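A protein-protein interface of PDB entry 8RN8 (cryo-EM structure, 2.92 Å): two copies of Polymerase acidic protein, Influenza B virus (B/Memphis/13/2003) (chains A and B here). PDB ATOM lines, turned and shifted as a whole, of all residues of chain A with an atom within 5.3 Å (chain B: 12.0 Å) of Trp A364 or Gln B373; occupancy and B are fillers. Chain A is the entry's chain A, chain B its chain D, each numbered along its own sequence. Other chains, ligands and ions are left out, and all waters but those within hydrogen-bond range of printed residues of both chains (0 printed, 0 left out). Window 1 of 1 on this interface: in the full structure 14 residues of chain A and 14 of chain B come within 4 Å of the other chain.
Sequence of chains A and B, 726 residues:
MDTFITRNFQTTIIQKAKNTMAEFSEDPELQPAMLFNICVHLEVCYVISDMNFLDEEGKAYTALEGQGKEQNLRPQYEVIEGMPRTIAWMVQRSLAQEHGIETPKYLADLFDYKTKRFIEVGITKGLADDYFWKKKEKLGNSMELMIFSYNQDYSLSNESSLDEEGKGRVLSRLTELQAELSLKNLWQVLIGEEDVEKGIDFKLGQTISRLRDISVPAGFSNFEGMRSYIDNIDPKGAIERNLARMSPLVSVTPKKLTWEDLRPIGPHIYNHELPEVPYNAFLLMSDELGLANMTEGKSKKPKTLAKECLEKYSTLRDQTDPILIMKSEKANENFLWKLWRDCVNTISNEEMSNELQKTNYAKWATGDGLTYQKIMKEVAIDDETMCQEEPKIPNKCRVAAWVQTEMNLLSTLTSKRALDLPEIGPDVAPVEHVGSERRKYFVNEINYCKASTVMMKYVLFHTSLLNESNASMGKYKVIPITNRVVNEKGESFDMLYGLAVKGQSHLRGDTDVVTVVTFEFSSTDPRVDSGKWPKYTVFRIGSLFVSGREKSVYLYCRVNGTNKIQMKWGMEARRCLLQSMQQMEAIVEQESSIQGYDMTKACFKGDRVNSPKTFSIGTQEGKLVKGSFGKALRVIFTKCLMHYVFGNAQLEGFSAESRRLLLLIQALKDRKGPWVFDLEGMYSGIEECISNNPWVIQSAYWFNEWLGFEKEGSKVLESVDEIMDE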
ATOM      1  N   PHE A 335      -1.095 -22.399  33.341  1.00  0.00           N
ATOM      2  CA  PHE A 335      -0.209 -22.931  32.310  1.00  0.00           C
ATOM      3  C   PHE A 335       1.249 -22.717  32.688  1.00  0.00           C
ATOM      4  O   PHE A 335       2.075 -23.630  32.571  1.00  0.00           O
ATOM      5  CB  PHE A 335      -0.506 -22.258  30.968  1.00  0.00           C
ATOM      6  CG  PHE A 335      -1.800 -22.689  30.325  1.00  0.00           C
ATOM      7  CD1 PHE A 335      -2.578 -23.699  30.866  1.00  0.00           C
ATOM      8  CD2 PHE A 335      -2.235 -22.074  29.165  1.00  0.00           C
ATOM      9  CE1 PHE A 335      -3.757 -24.081  30.261  1.00  0.00           C
ATOM     10  CE2 PHE A 335      -3.413 -22.455  28.560  1.00  0.00           C
ATOM     11  CZ  PHE A 335      -4.174 -23.458  29.109  1.00  0.00           C
ATOM     12  N   ASN A 360       2.043 -32.757  25.267  1.00  0.00           N
ATOM     13  CA  ASN A 360       0.735 -32.309  24.802  1.00  0.00           C
ATOM     14  C   ASN A 360       0.236 -31.122  25.614  1.00  0.00           C
ATOM     15  O   ASN A 360      -0.303 -30.161  25.053  1.00  0.00           O
ATOM     16  CB  ASN A 360      -0.267 -33.460  24.867  1.00  0.00           C
ATOM     17  CG  ASN A 360      -0.139 -34.407  23.695  1.00  0.00           C
ATOM     18  OD1 ASN A 360       0.565 -35.413  23.769  1.00  0.00           O
ATOM     19  ND2 ASN A 360      -0.815 -34.086  22.598  1.00  0.00           N
ATOM     20  N   TYR A 361       0.396 -31.169  26.937  1.00  0.00           N
ATOM     21  CA  TYR A 361       0.008 -30.027  27.756  1.00  0.00           C
ATOM     22  C   TYR A 361       0.878 -28.816  27.452  1.00  0.00           C
ATOM     23  O   TYR A 361       0.378 -27.688  27.375  1.00  0.00           O
ATOM     24  CB  TYR A 361       0.091 -30.381  29.238  1.00  0.00           C
ATOM     25  CG  TYR A 361      -0.416 -29.281  30.137  1.00  0.00           C
ATOM     26  CD1 TYR A 361      -1.762 -29.184  30.455  1.00  0.00           C
ATOM     27  CD2 TYR A 361       0.448 -28.328  30.657  1.00  0.00           C
ATOM     28  CE1 TYR A 361      -2.233 -28.175  31.268  1.00  0.00           C
ATOM     29  CE2 TYR A 361      -0.014 -27.317  31.472  1.00  0.00           C
ATOM     30  CZ  TYR A 361      -1.354 -27.246  31.774  1.00  0.00           C
ATOM     31  OH  TYR A 361      -1.819 -26.240  32.585  1.00  0.00           O
ATOM     32  N   ALA A 362       2.185 -29.029  27.280  1.00  0.00           N
ATOM     33  CA  ALA A 362       3.085 -27.927  26.967  1.00  0.00           C
ATOM     34  C   ALA A 362       2.773 -27.303  25.616  1.00  0.00           C
ATOM     35  O   ALA A 362       3.150 -26.151  25.376  1.00  0.00           O
ATOM     36  CB  ALA A 362       4.534 -28.410  26.996  1.00  0.00           C
ATOM     37  N   LYS A 363       2.095 -28.032  24.730  1.00  0.00           N
ATOM     38  CA  LYS A 363       1.707 -27.452  23.449  1.00  0.00           C
ATOM     39  C   LYS A 363       0.789 -26.254  23.648  1.00  0.00           C
ATOM     40  O   LYS A 363       0.912 -25.246  22.944  1.00  0.00           O
ATOM     41  CB  LYS A 363       1.025 -28.508  22.580  1.00  0.00           C
ATOM     42  CG  LYS A 363       0.684 -28.031  21.176  1.00  0.00           C
ATOM     43  CD  LYS A 363      -0.453 -28.833  20.573  1.00  0.00           C
ATOM     44  CE  LYS A 363      -0.949 -28.199  19.286  1.00  0.00           C
ATOM     45  NZ  LYS A 363      -1.960 -29.045  18.595  1.00  0.00           N
ATOM     46  N   TRP A 364      -0.144 -26.350  24.594  1.00  0.00           N
ATOM     47  CA  TRP A 364      -1.081 -25.267  24.857  1.00  0.00           C
ATOM     48  C   TRP A 364      -0.610 -24.337  25.963  1.00  0.00           C
ATOM     49  O   TRP A 364      -1.001 -23.165  25.982  1.00  0.00           O
ATOM     50  CB  TRP A 364      -2.452 -25.839  25.226  1.00  0.00           C
ATOM     51  CG  TRP A 364      -3.022 -26.705  24.154  1.00  0.00           C
ATOM     52  CD1 TRP A 364      -3.017 -28.065  24.112  1.00  0.00           C
ATOM     53  CD2 TRP A 364      -3.670 -26.267  22.958  1.00  0.00           C
ATOM     54  NE1 TRP A 364      -3.624 -28.504  22.964  1.00  0.00           N
ATOM     55  CE2 TRP A 364      -4.034 -27.418  22.237  1.00  0.00           C
ATOM     56  CE3 TRP A 364      -3.978 -25.014  22.425  1.00  0.00           C
ATOM     57  CZ2 TRP A 364      -4.690 -27.355  21.013  1.00  0.00           C
ATOM     58  CZ3 TRP A 364      -4.631 -24.953  21.212  1.00  0.00           C
ATOM     59  CH2 TRP A 364      -4.981 -26.115  20.519  1.00  0.00           C
ATOM     60  N   ALA A 365       0.217 -24.830  26.885  1.00  0.00           N
ATOM     61  CA  ALA A 365       0.718 -23.970  27.951  1.00  0.00           C
ATOM     62  C   ALA A 365       1.565 -22.838  27.388  1.00  0.00           C
ATOM     63  O   ALA A 365       1.483 -21.697  27.858  1.00  0.00           O
ATOM     64  CB  ALA A 365       1.522 -24.794  28.954  1.00  0.00           C
ATOM     65  N   THR A 366       2.385 -23.132  26.382  1.00  0.00           N
ATOM     66  CA  THR A 366       3.220 -22.130  25.739  1.00  0.00           C
ATOM     67  C   THR A 366       2.469 -21.304  24.703  1.00  0.00           C
ATOM     68  O   THR A 366       3.016 -20.313  24.211  1.00  0.00           O
ATOM     69  CB  THR A 366       4.420 -22.799  25.061  1.00  0.00           C
ATOM     70  OG1 THR A 366       3.968 -23.593  23.959  1.00  0.00           O
ATOM     71  CG2 THR A 366       5.169 -23.684  26.045  1.00  0.00           C
ATOM     72  N   GLY A 367       1.238 -21.679  24.367  1.00  0.00           N
ATOM     73  CA  GLY A 367       0.490 -20.984  23.343  1.00  0.00           C
ATOM     74  C   GLY A 367       0.820 -21.391  21.928  1.00  0.00           C
ATOM     75  O   GLY A 367       0.387 -20.715  20.990  1.00  0.00           O
ATOM     76  N   ASP A 368       1.578 -22.474  21.740  1.00  0.00           N
ATOM     77  CA  ASP A 368       1.939 -22.908  20.398  1.00  0.00           C
ATOM     78  C   ASP A 368       0.745 -23.438  19.619  1.00  0.00           C
ATOM     79  O   ASP A 368       0.761 -23.401  18.385  1.00  0.00           O
ATOM     80  CB  ASP A 368       3.022 -23.984  20.467  1.00  0.00           C
ATOM     81  CG  ASP A 368       4.419 -23.403  20.546  1.00  0.00           C
ATOM     82  OD1 ASP A 368       4.546 -22.165  20.638  1.00  0.00           O
ATOM     83  OD2 ASP A 368       5.392 -24.186  20.510  1.00  0.00           O
ATOM     84  N   GLY A 369      -0.285 -23.939  20.305  1.00  0.00           N
ATOM     85  CA  GLY A 369      -1.460 -24.437  19.615  1.00  0.00           C
ATOM     86  C   GLY A 369      -2.337 -23.350  19.034  1.00  0.00           C
ATOM     87  O   GLY A 369      -3.116 -23.624  18.115  1.00  0.00           O
ATOM     88  N   LEU A 370      -2.225 -22.127  19.540  1.00  0.00           N
ATOM     89  CA  LEU A 370      -3.035 -21.005  19.068  1.00  0.00           C
ATOM     90  C   LEU A 370      -2.387 -20.312  17.873  1.00  0.00           C
ATOM     91  O   LEU A 370      -2.170 -19.103  17.874  1.00  0.00           O
ATOM     92  CB  LEU A 370      -3.261 -20.018  20.208  1.00  0.00           C
ATOM     93  CG  LEU A 370      -4.202 -20.417  21.347  1.00  0.00           C
ATOM     94  CD1 LEU A 370      -4.658 -19.175  22.090  1.00  0.00           C
ATOM     95  CD2 LEU A 370      -5.405 -21.200  20.849  1.00  0.00           C
ATOM     96  N   LYS B 363     -13.873 -27.738   1.200  1.00  0.00           N
ATOM     97  CA  LYS B 363     -13.651 -27.866   2.635  1.00  0.00           C
ATOM     98  C   LYS B 363     -14.027 -26.588   3.370  1.00  0.00           C
ATOM     99  O   LYS B 363     -14.459 -26.642   4.526  1.00  0.00           O
ATOM    100  CB  LYS B 363     -12.191 -28.226   2.907  1.00  0.00           C
ATOM    101  CG  LYS B 363     -11.866 -28.491   4.368  1.00  0.00           C
ATOM    102  CD  LYS B 363     -10.402 -28.219   4.661  1.00  0.00           C
ATOM    103  CE  LYS B 363      -9.911 -29.009   5.861  1.00  0.00           C
ATOM    104  NZ  LYS B 363     -10.399 -28.438   7.144  1.00  0.00           N
ATOM    105  N   TRP B 364     -13.868 -25.436   2.722  1.00  0.00           N
ATOM    106  CA  TRP B 364     -14.207 -24.151   3.317  1.00  0.00           C
ATOM    107  C   TRP B 364     -15.477 -23.541   2.754  1.00  0.00           C
ATOM    108  O   TRP B 364     -16.135 -22.769   3.454  1.00  0.00           O
ATOM    109  CB  TRP B 364     -13.050 -23.163   3.126  1.00  0.00           C
ATOM    110  CG  TRP B 364     -11.761 -23.688   3.660  1.00  0.00           C
ATOM    111  CD1 TRP B 364     -10.786 -24.331   2.961  1.00  0.00           C
ATOM    112  CD2 TRP B 364     -11.311 -23.628   5.017  1.00  0.00           C
ATOM    113  NE1 TRP B 364      -9.752 -24.672   3.796  1.00  0.00           N
ATOM    114  CE2 TRP B 364     -10.050 -24.252   5.065  1.00  0.00           C
ATOM    115  CE3 TRP B 364     -11.849 -23.106   6.194  1.00  0.00           C
ATOM    116  CZ2 TRP B 364      -9.322 -24.366   6.242  1.00  0.00           C
ATOM    117  CZ3 TRP B 364     -11.124 -23.221   7.360  1.00  0.00           C
ATOM    118  CH2 TRP B 364      -9.874 -23.846   7.377  1.00  0.00           C
ATOM    119  N   GLY B 367     -18.121 -24.797   4.856  1.00  0.00           N
ATOM    120  CA  GLY B 367     -17.935 -24.517   6.263  1.00  0.00           C
ATOM    121  C   GLY B 367     -17.404 -25.675   7.072  1.00  0.00           C
ATOM    122  O   GLY B 367     -17.415 -25.605   8.306  1.00  0.00           O
ATOM    123  N   ASP B 368     -16.944 -26.744   6.419  1.00  0.00           N
ATOM    124  CA  ASP B 368     -16.418 -27.891   7.151  1.00  0.00           C
ATOM    125  C   ASP B 368     -15.159 -27.522   7.924  1.00  0.00           C
ATOM    126  O   ASP B 368     -14.963 -27.974   9.058  1.00  0.00           O
ATOM    127  CB  ASP B 368     -16.130 -29.039   6.186  1.00  0.00           C
ATOM    128  CG  ASP B 368     -17.382 -29.787   5.777  1.00  0.00           C
ATOM    129  OD1 ASP B 368     -18.473 -29.447   6.277  1.00  0.00           O
ATOM    130  OD2 ASP B 368     -17.273 -30.717   4.952  1.00  0.00           O
ATOM    131  N   GLY B 369     -14.291 -26.704   7.327  1.00  0.00           N
ATOM    132  CA  GLY B 369     -13.024 -26.378   7.956  1.00  0.00           C
ATOM    133  C   GLY B 369     -13.146 -25.491   9.175  1.00  0.00           C
ATOM    134  O   GLY B 369     -12.210 -25.433   9.978  1.00  0.00           O
ATOM    135  N   LEU B 370     -14.271 -24.802   9.334  1.00  0.00           N
ATOM    136  CA  LEU B 370     -14.474 -23.897  10.466  1.00  0.00           C
ATOM    137  C   LEU B 370     -15.019 -24.646  11.678  1.00  0.00           C
ATOM    138  O   LEU B 370     -16.030 -24.271  12.269  1.00  0.00           O
ATOM    139  CB  LEU B 370     -15.411 -22.765  10.057  1.00  0.00           C
ATOM    140  CG  LEU B 370     -14.847 -21.476   9.448  1.00  0.00           C
ATOM    141  CD1 LEU B 370     -15.812 -20.335   9.729  1.00  0.00           C
ATOM    142  CD2 LEU B 370     -13.447 -21.126   9.939  1.00  0.00           C
ATOM    143  N   THR B 371     -14.337 -25.719  12.065  1.00  0.00           N
ATOM    144  CA  THR B 371     -14.777 -26.586  13.147  1.00  0.00           C
ATOM    145  C   THR B 371     -13.825 -26.464  14.328  1.00  0.00           C
ATOM    146  O   THR B 371     -12.603 -26.423  14.153  1.00  0.00           O
ATOM    147  CB  THR B 371     -14.857 -28.044  12.685  1.00  0.00           C
ATOM    148  OG1 THR B 371     -15.567 -28.821  13.656  1.00  0.00           O
ATOM    149  CG2 THR B 371     -13.465 -28.627  12.487  1.00  0.00           C
ATOM    150  N   TYR B 372     -14.393 -26.402  15.531  1.00  0.00           N
ATOM    151  CA  TYR B 372     -13.586 -26.255  16.732  1.00  0.00           C
ATOM    152  C   TYR B 372     -12.681 -27.466  16.918  1.00  0.00           C
ATOM    153  O   TYR B 372     -13.034 -28.596  16.569  1.00  0.00           O
ATOM    154  CB  TYR B 372     -14.482 -26.079  17.957  1.00  0.00           C
ATOM    155  CG  TYR B 372     -15.088 -24.700  18.098  1.00  0.00           C
ATOM    156  CD1 TYR B 372     -15.215 -23.856  17.004  1.00  0.00           C
ATOM    157  CD2 TYR B 372     -15.542 -24.245  19.328  1.00  0.00           C
ATOM    158  CE1 TYR B 372     -15.770 -22.602  17.132  1.00  0.00           C
ATOM    159  CE2 TYR B 372     -16.099 -22.992  19.465  1.00  0.00           C
ATOM    160  CZ  TYR B 372     -16.210 -22.175  18.364  1.00  0.00           C
ATOM    161  OH  TYR B 372     -16.765 -20.925  18.493  1.00  0.00           O
ATOM    162  N   GLN B 373     -11.502 -27.221  17.477  1.00  0.00           N
ATOM    163  CA  GLN B 373     -10.501 -28.257  17.693  1.00  0.00           C
ATOM    164  C   GLN B 373     -10.597 -28.769  19.123  1.00  0.00           C
ATOM    165  O   GLN B 373     -10.637 -27.977  20.069  1.00  0.00           O
ATOM    166  CB  GLN B 373      -9.097 -27.717  17.417  1.00  0.00           C
ATOM    167  CG  GLN B 373      -7.991 -28.446  18.157  1.00  0.00           C
ATOM    168  CD  GLN B 373      -6.649 -28.306  17.474  1.00  0.00           C
ATOM    169  OE1 GLN B 373      -6.148 -29.253  16.869  1.00  0.00           O
ATOM    170  NE2 GLN B 373      -6.059 -27.120  17.565  1.00  0.00           N
ATOM    171  N   LYS B 374     -10.633 -30.090  19.275  1.00  0.00           N
ATOM    172  CA  LYS B 374     -10.714 -30.695  20.593  1.00  0.00           C
ATOM    173  C   LYS B 374      -9.341 -30.735  21.246  1.00  0.00           C
ATOM    174  O   LYS B 374      -8.333 -31.021  20.593  1.00  0.00           O
ATOM    175  CB  LYS B 374     -11.285 -32.110  20.501  1.00  0.00           C
ATOM    176  CG  LYS B 374     -12.312 -32.420  21.576  1.00  0.00           C
ATOM    177  CD  LYS B 374     -12.705 -33.886  21.571  1.00  0.00           C
ATOM    178  CE  LYS B 374     -13.207 -34.330  22.936  1.00  0.00           C
ATOM    179  NZ  LYS B 374     -12.133 -34.319  23.967  1.00  0.00           N
ATOM    180  N   ILE B 375      -9.306 -30.446  22.545  1.00  0.00           N
ATOM    181  CA  ILE B 375      -8.076 -30.465  23.322  1.00  0.00           C
ATOM    182  C   ILE B 375      -8.310 -31.306  24.566  1.00  0.00           C
ATOM    183  O   ILE B 375      -9.444 -31.459  25.028  1.00  0.00           O
ATOM    184  CB  ILE B 375      -7.611 -29.041  23.697  1.00  0.00           C
ATOM    185  CG1 ILE B 375      -8.596 -28.382  24.665  1.00  0.00           C
ATOM    186  CG2 ILE B 375      -7.478 -28.197  22.449  1.00  0.00           C
ATOM    187  CD1 ILE B 375      -8.202 -26.980  25.072  1.00  0.00           C
ATOM    188  N   MET B 376      -7.226 -31.855  25.110  1.00  0.00           N
ATOM    189  CA  MET B 376      -7.344 -32.699  26.289  1.00  0.00           C
ATOM    190  C   MET B 376      -8.033 -31.937  27.416  1.00  0.00           C
ATOM    191  O   MET B 376      -8.031 -30.706  27.467  1.00  0.00           O
ATOM    192  CB  MET B 376      -5.972 -33.192  26.750  1.00  0.00           C
ATOM    193  CG  MET B 376      -4.857 -32.172  26.638  1.00  0.00           C
ATOM    194  SD  MET B 376      -3.616 -32.375  27.929  1.00  0.00           S
ATOM    195  CE  MET B 376      -2.804 -33.870  27.379  1.00  0.00           C
ATOM    196  N   LYS B 377      -8.638 -32.697  28.329  1.00  0.00           N
ATOM    197  CA  LYS B 377      -9.459 -32.087  29.368  1.00  0.00           C
ATOM    198  C   LYS B 377      -8.634 -31.164  30.257  1.00  0.00           C
ATOM    199  O   LYS B 377      -9.101 -30.087  30.636  1.00  0.00           O
ATOM    200  CB  LYS B 377     -10.144 -33.167  30.205  1.00  0.00           C
ATOM    201  CG  LYS B 377      -9.213 -34.246  30.737  1.00  0.00           C
ATOM    202  CD  LYS B 377      -9.975 -35.302  31.521  1.00  0.00           C
ATOM    203  CE  LYS B 377     -10.314 -34.828  32.924  1.00  0.00           C
ATOM    204  NZ  LYS B 377      -9.101 -34.586  33.751  1.00  0.00           N
ATOM    205  N   GLU B 378      -7.402 -31.560  30.584  1.00  0.00           N
ATOM    206  CA  GLU B 378      -6.611 -30.810  31.556  1.00  0.00           C
ATOM    207  C   GLU B 378      -6.415 -29.362  31.122  1.00  0.00           C
ATOM    208  O   GLU B 378      -6.562 -28.436  31.931  1.00  0.00           O
ATOM    209  CB  GLU B 378      -5.260 -31.494  31.755  1.00  0.00           C
ATOM    210  CG  GLU B 378      -4.705 -31.382  33.163  1.00  0.00           C
ATOM    211  CD  GLU B 378      -3.210 -31.624  33.213  1.00  0.00           C
ATOM    212  OE1 GLU B 378      -2.743 -32.586  32.569  1.00  0.00           O
ATOM    213  OE2 GLU B 378      -2.502 -30.854  33.894  1.00  0.00           O
ATOM    214  N   VAL B 379      -6.087 -29.144  29.848  1.00  0.00           N
ATOM    215  CA  VAL B 379      -5.893 -27.784  29.358  1.00  0.00           C
ATOM    216  C   VAL B 379      -7.179 -26.982  29.501  1.00  0.00           C
ATOM    217  O   VAL B 379      -7.162 -25.820  29.920  1.00  0.00           O
ATOM    218  CB  VAL B 379      -5.398 -27.805  27.899  1.00  0.00           C
ATOM    219  CG1 VAL B 379      -5.020 -26.408  27.449  1.00  0.00           C
ATOM    220  CG2 VAL B 379      -4.207 -28.737  27.750  1.00  0.00           C
ATOM    221  N   ALA B 380      -8.314 -27.590  29.155  1.00  0.00           N
ATOM    222  CA  ALA B 380      -9.588 -26.884  29.238  1.00  0.00           C
ATOM    223  C   ALA B 380      -9.928 -26.525  30.678  1.00  0.00           C
ATOM    224  O   ALA B 380     -10.443 -25.436  30.949  1.00  0.00           O
ATOM    225  CB  ALA B 380     -10.692 -27.735  28.620  1.00  0.00           C
ATOM    226  N   ILE B 381      -9.657 -27.434  31.615  1.00  0.00           N
ATOM    227  CA  ILE B 381      -9.881 -27.129  33.025  1.00  0.00           C
ATOM    228  C   ILE B 381      -9.003 -25.965  33.458  1.00  0.00           C
ATOM    229  O   ILE B 381      -9.450 -25.068  34.182  1.00  0.00           O
ATOM    230  CB  ILE B 381      -9.642 -28.379  33.893  1.00  0.00           C
ATOM    231  CG1 ILE B 381     -10.444 -29.564  33.342  1.00  0.00           C
ATOM    232  CG2 ILE B 381      -9.982 -28.097  35.356  1.00  0.00           C
ATOM    233  CD1 ILE B 381     -10.807 -30.612  34.368  1.00  0.00           C
ATOM    234  N   ASP B 382      -7.737 -25.962  33.035  1.00  0.00           N
ATOM    235  CA  ASP B 382      -6.864 -24.843  33.373  1.00  0.00           C
ATOM    236  C   ASP B 382      -7.323 -23.556  32.696  1.00  0.00           C
ATOM    237  O   ASP B 382      -7.310 -22.485  33.314  1.00  0.00           O
ATOM    238  CB  ASP B 382      -5.423 -25.166  32.986  1.00  0.00           C
ATOM    239  CG  ASP B 382      -4.770 -26.142  33.939  1.00  0.00           C
ATOM    240  OD1 ASP B 382      -5.248 -26.272  35.084  1.00  0.00           O
ATOM    241  OD2 ASP B 382      -3.773 -26.778  33.543  1.00  0.00           O
ATOM    242  N   ASP B 383      -7.736 -23.638  31.434  1.00  0.00           N
ATOM    243  CA  ASP B 383      -8.110 -22.453  30.668  1.00  0.00           C
ATOM    244  C   ASP B 383      -9.379 -21.846  31.253  1.00  0.00           C
ATOM    245  O   ASP B 383     -10.447 -22.465  31.220  1.00  0.00           O
ATOM    246  CB  ASP B 383      -8.303 -22.820  29.201  1.00  0.00           C
ATOM    247  CG  ASP B 383      -8.314 -21.608  28.294  1.00  0.00           C
ATOM    248  OD1 ASP B 383      -8.494 -20.484  28.803  1.00  0.00           O
ATOM    249  OD2 ASP B 383      -8.135 -21.779  27.071  1.00  0.00           O
ATOM    250  N   GLU B 384      -9.265 -20.628  31.785  1.00  0.00           N
ATOM    251  CA  GLU B 384     -10.388 -19.969  32.438  1.00  0.00           C
ATOM    252  C   GLU B 384     -11.395 -19.397  31.449  1.00  0.00           C
ATOM    253  O   GLU B 384     -12.560 -19.212  31.815  1.00  0.00           O
ATOM    254  CB  GLU B 384      -9.862 -18.863  33.360  1.00  0.00           C
ATOM    255  CG  GLU B 384     -10.884 -17.819  33.804  1.00  0.00           C
ATOM    256  CD  GLU B 384     -10.229 -16.608  34.437  1.00  0.00           C
ATOM    257  OE1 GLU B 384      -9.516 -15.876  33.720  1.00  0.00           O
ATOM    258  OE2 GLU B 384     -10.426 -16.388  35.651  1.00  0.00           O
ATOM    259  N   THR B 385     -10.982 -19.112  30.216  1.00  0.00           N
ATOM    260  CA  THR B 385     -11.887 -18.527  29.235  1.00  0.00           C
ATOM    261  C   THR B 385     -12.803 -19.555  28.587  1.00  0.00           C
ATOM    262  O   THR B 385     -13.689 -19.170  27.818  1.00  0.00           O
ATOM    263  CB  THR B 385     -11.093 -17.802  28.146  1.00  0.00           C
ATOM    264  OG1 THR B 385     -10.529 -18.758  27.241  1.00  0.00           O
ATOM    265  CG2 THR B 385      -9.982 -16.962  28.757  1.00  0.00           C
ATOM    266  N   MET B 386     -12.615 -20.839  28.873  1.00  0.00           N
ATOM    267  CA  MET B 386     -13.448 -21.895  28.318  1.00  0.00           C
ATOM    268  C   MET B 386     -14.669 -22.085  29.209  1.00  0.00           C
ATOM    269  O   MET B 386     -14.539 -22.502  30.364  1.00  0.00           O
ATOM    270  CB  MET B 386     -12.660 -23.196  28.211  1.00  0.00           C
ATOM    271  CG  MET B 386     -12.009 -23.416  26.868  1.00  0.00           C
ATOM    272  SD  MET B 386     -11.206 -25.021  26.776  1.00  0.00           S
ATOM    273  CE  MET B 386     -11.183 -25.277  25.013  1.00  0.00           C
ATOM    274  N   CYS B 387     -15.849 -21.782  28.674  1.00  0.00           N
ATOM    275  CA  CYS B 387     -17.089 -21.891  29.425  1.00  0.00           C
ATOM    276  C   CYS B 387     -18.158 -22.521  28.545  1.00  0.00           C
ATOM    277  O   CYS B 387     -18.102 -22.452  27.316  1.00  0.00           O
ATOM    278  CB  CYS B 387     -17.562 -20.523  29.932  1.00  0.00           C
ATOM    279  SG  CYS B 387     -17.593 -19.233  28.672  1.00  0.00           S
ATOM    280  N   GLU B 389     -21.498 -23.085  26.541  1.00  0.00           N
ATOM    281  CA  GLU B 389     -22.300 -22.171  25.741  1.00  0.00           C
ATOM    282  C   GLU B 389     -23.751 -22.177  26.204  1.00  0.00           C
ATOM    283  O   GLU B 389     -24.259 -23.175  26.722  1.00  0.00           O
ATOM    284  CB  GLU B 389     -22.240 -22.540  24.258  1.00  0.00           C
ATOM    285  CG  GLU B 389     -20.947 -23.190  23.809  1.00  0.00           C
ATOM    286  CD  GLU B 389     -20.841 -23.275  22.299  1.00  0.00           C
ATOM    287  OE1 GLU B 389     -21.349 -22.363  21.615  1.00  0.00           O
ATOM    288  OE2 GLU B 389     -20.251 -24.253  21.795  1.00  0.00           O
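6 positions are printed for both chains.
The side-chain hydroxyl of Tyr A361 lies close to the side-chain carboxylate of Asp B382, at 2.2 Å.
Of the 12 printed residues of chain A, 4 touch a printed residue of chain B.
Hydrophobic or aromatic side chains of chain A within 4 Å of the printed part of chain B: Phe A335, Tyr A361 and Trp A364.
Among the printed residues, 9 pairs touch across the chains.
Among the printed residues, no Asp or Glu carboxylate lies within 4 Å of a Lys or Arg side-chain nitrogen of the other chain.
Of the printed residues of chain B, Trp A364 touches Gln B373, Ile B375 and Val B379.
Of chain A, only Trp A364 comes within 4 Å of Gln B373.
Tyr A361 touches three residues of chain B.
No residue of chain B comes within 4 Å of Ala A362.
No residue of chain B comes within 4 Å of Lys A363.
No residue of chain B comes within 4 Å of Thr A366.
No residue of chain B comes within 4 Å of Gly A367.
No residue of chain B comes within 4 Å of Asp A368.
Gly A369 touches none of the printed residues of chain B.
No residue of chain B comes within 4 Å of Leu A370.
Of the printed residues of chain A, Asp B382 touches Phe A335 (3.4 Å) and Tyr A361 (2.2 Å).
Of the printed residues of chain A, Ile B375 touches Trp A364 (3.2 Å).
Of the printed residues of chain A, Val B379 touches Phe A335, Tyr A361 and Trp A364.
Of the printed residues of chain A, Glu B378 touches Tyr A361 (3.8 Å).
Printed residues of chain B within 4 Å of Asn A360: Met B376.
Asp B383 touches none of the printed residues of chain A.
The nearest printed residue of chain A that does not touch Asp B382 is Ala A365 (7.3 Å).
Among the printed residues, pairs that only touch across the chains: Phe A335 with Val B379 (3.5 Å), Phe A335 with Asp B382 (3.4 Å), Asn A360 with Met B376 (3.6 Å), Tyr A361 with Glu B378 (3.8 Å), Tyr A361 with Val B379 (3.7 Å), Trp A364 with Gln B373 (3.3 Å), Trp A364 with Ile B375 (3.2 Å) and Trp A364 with Val B379 (3.4 Å).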
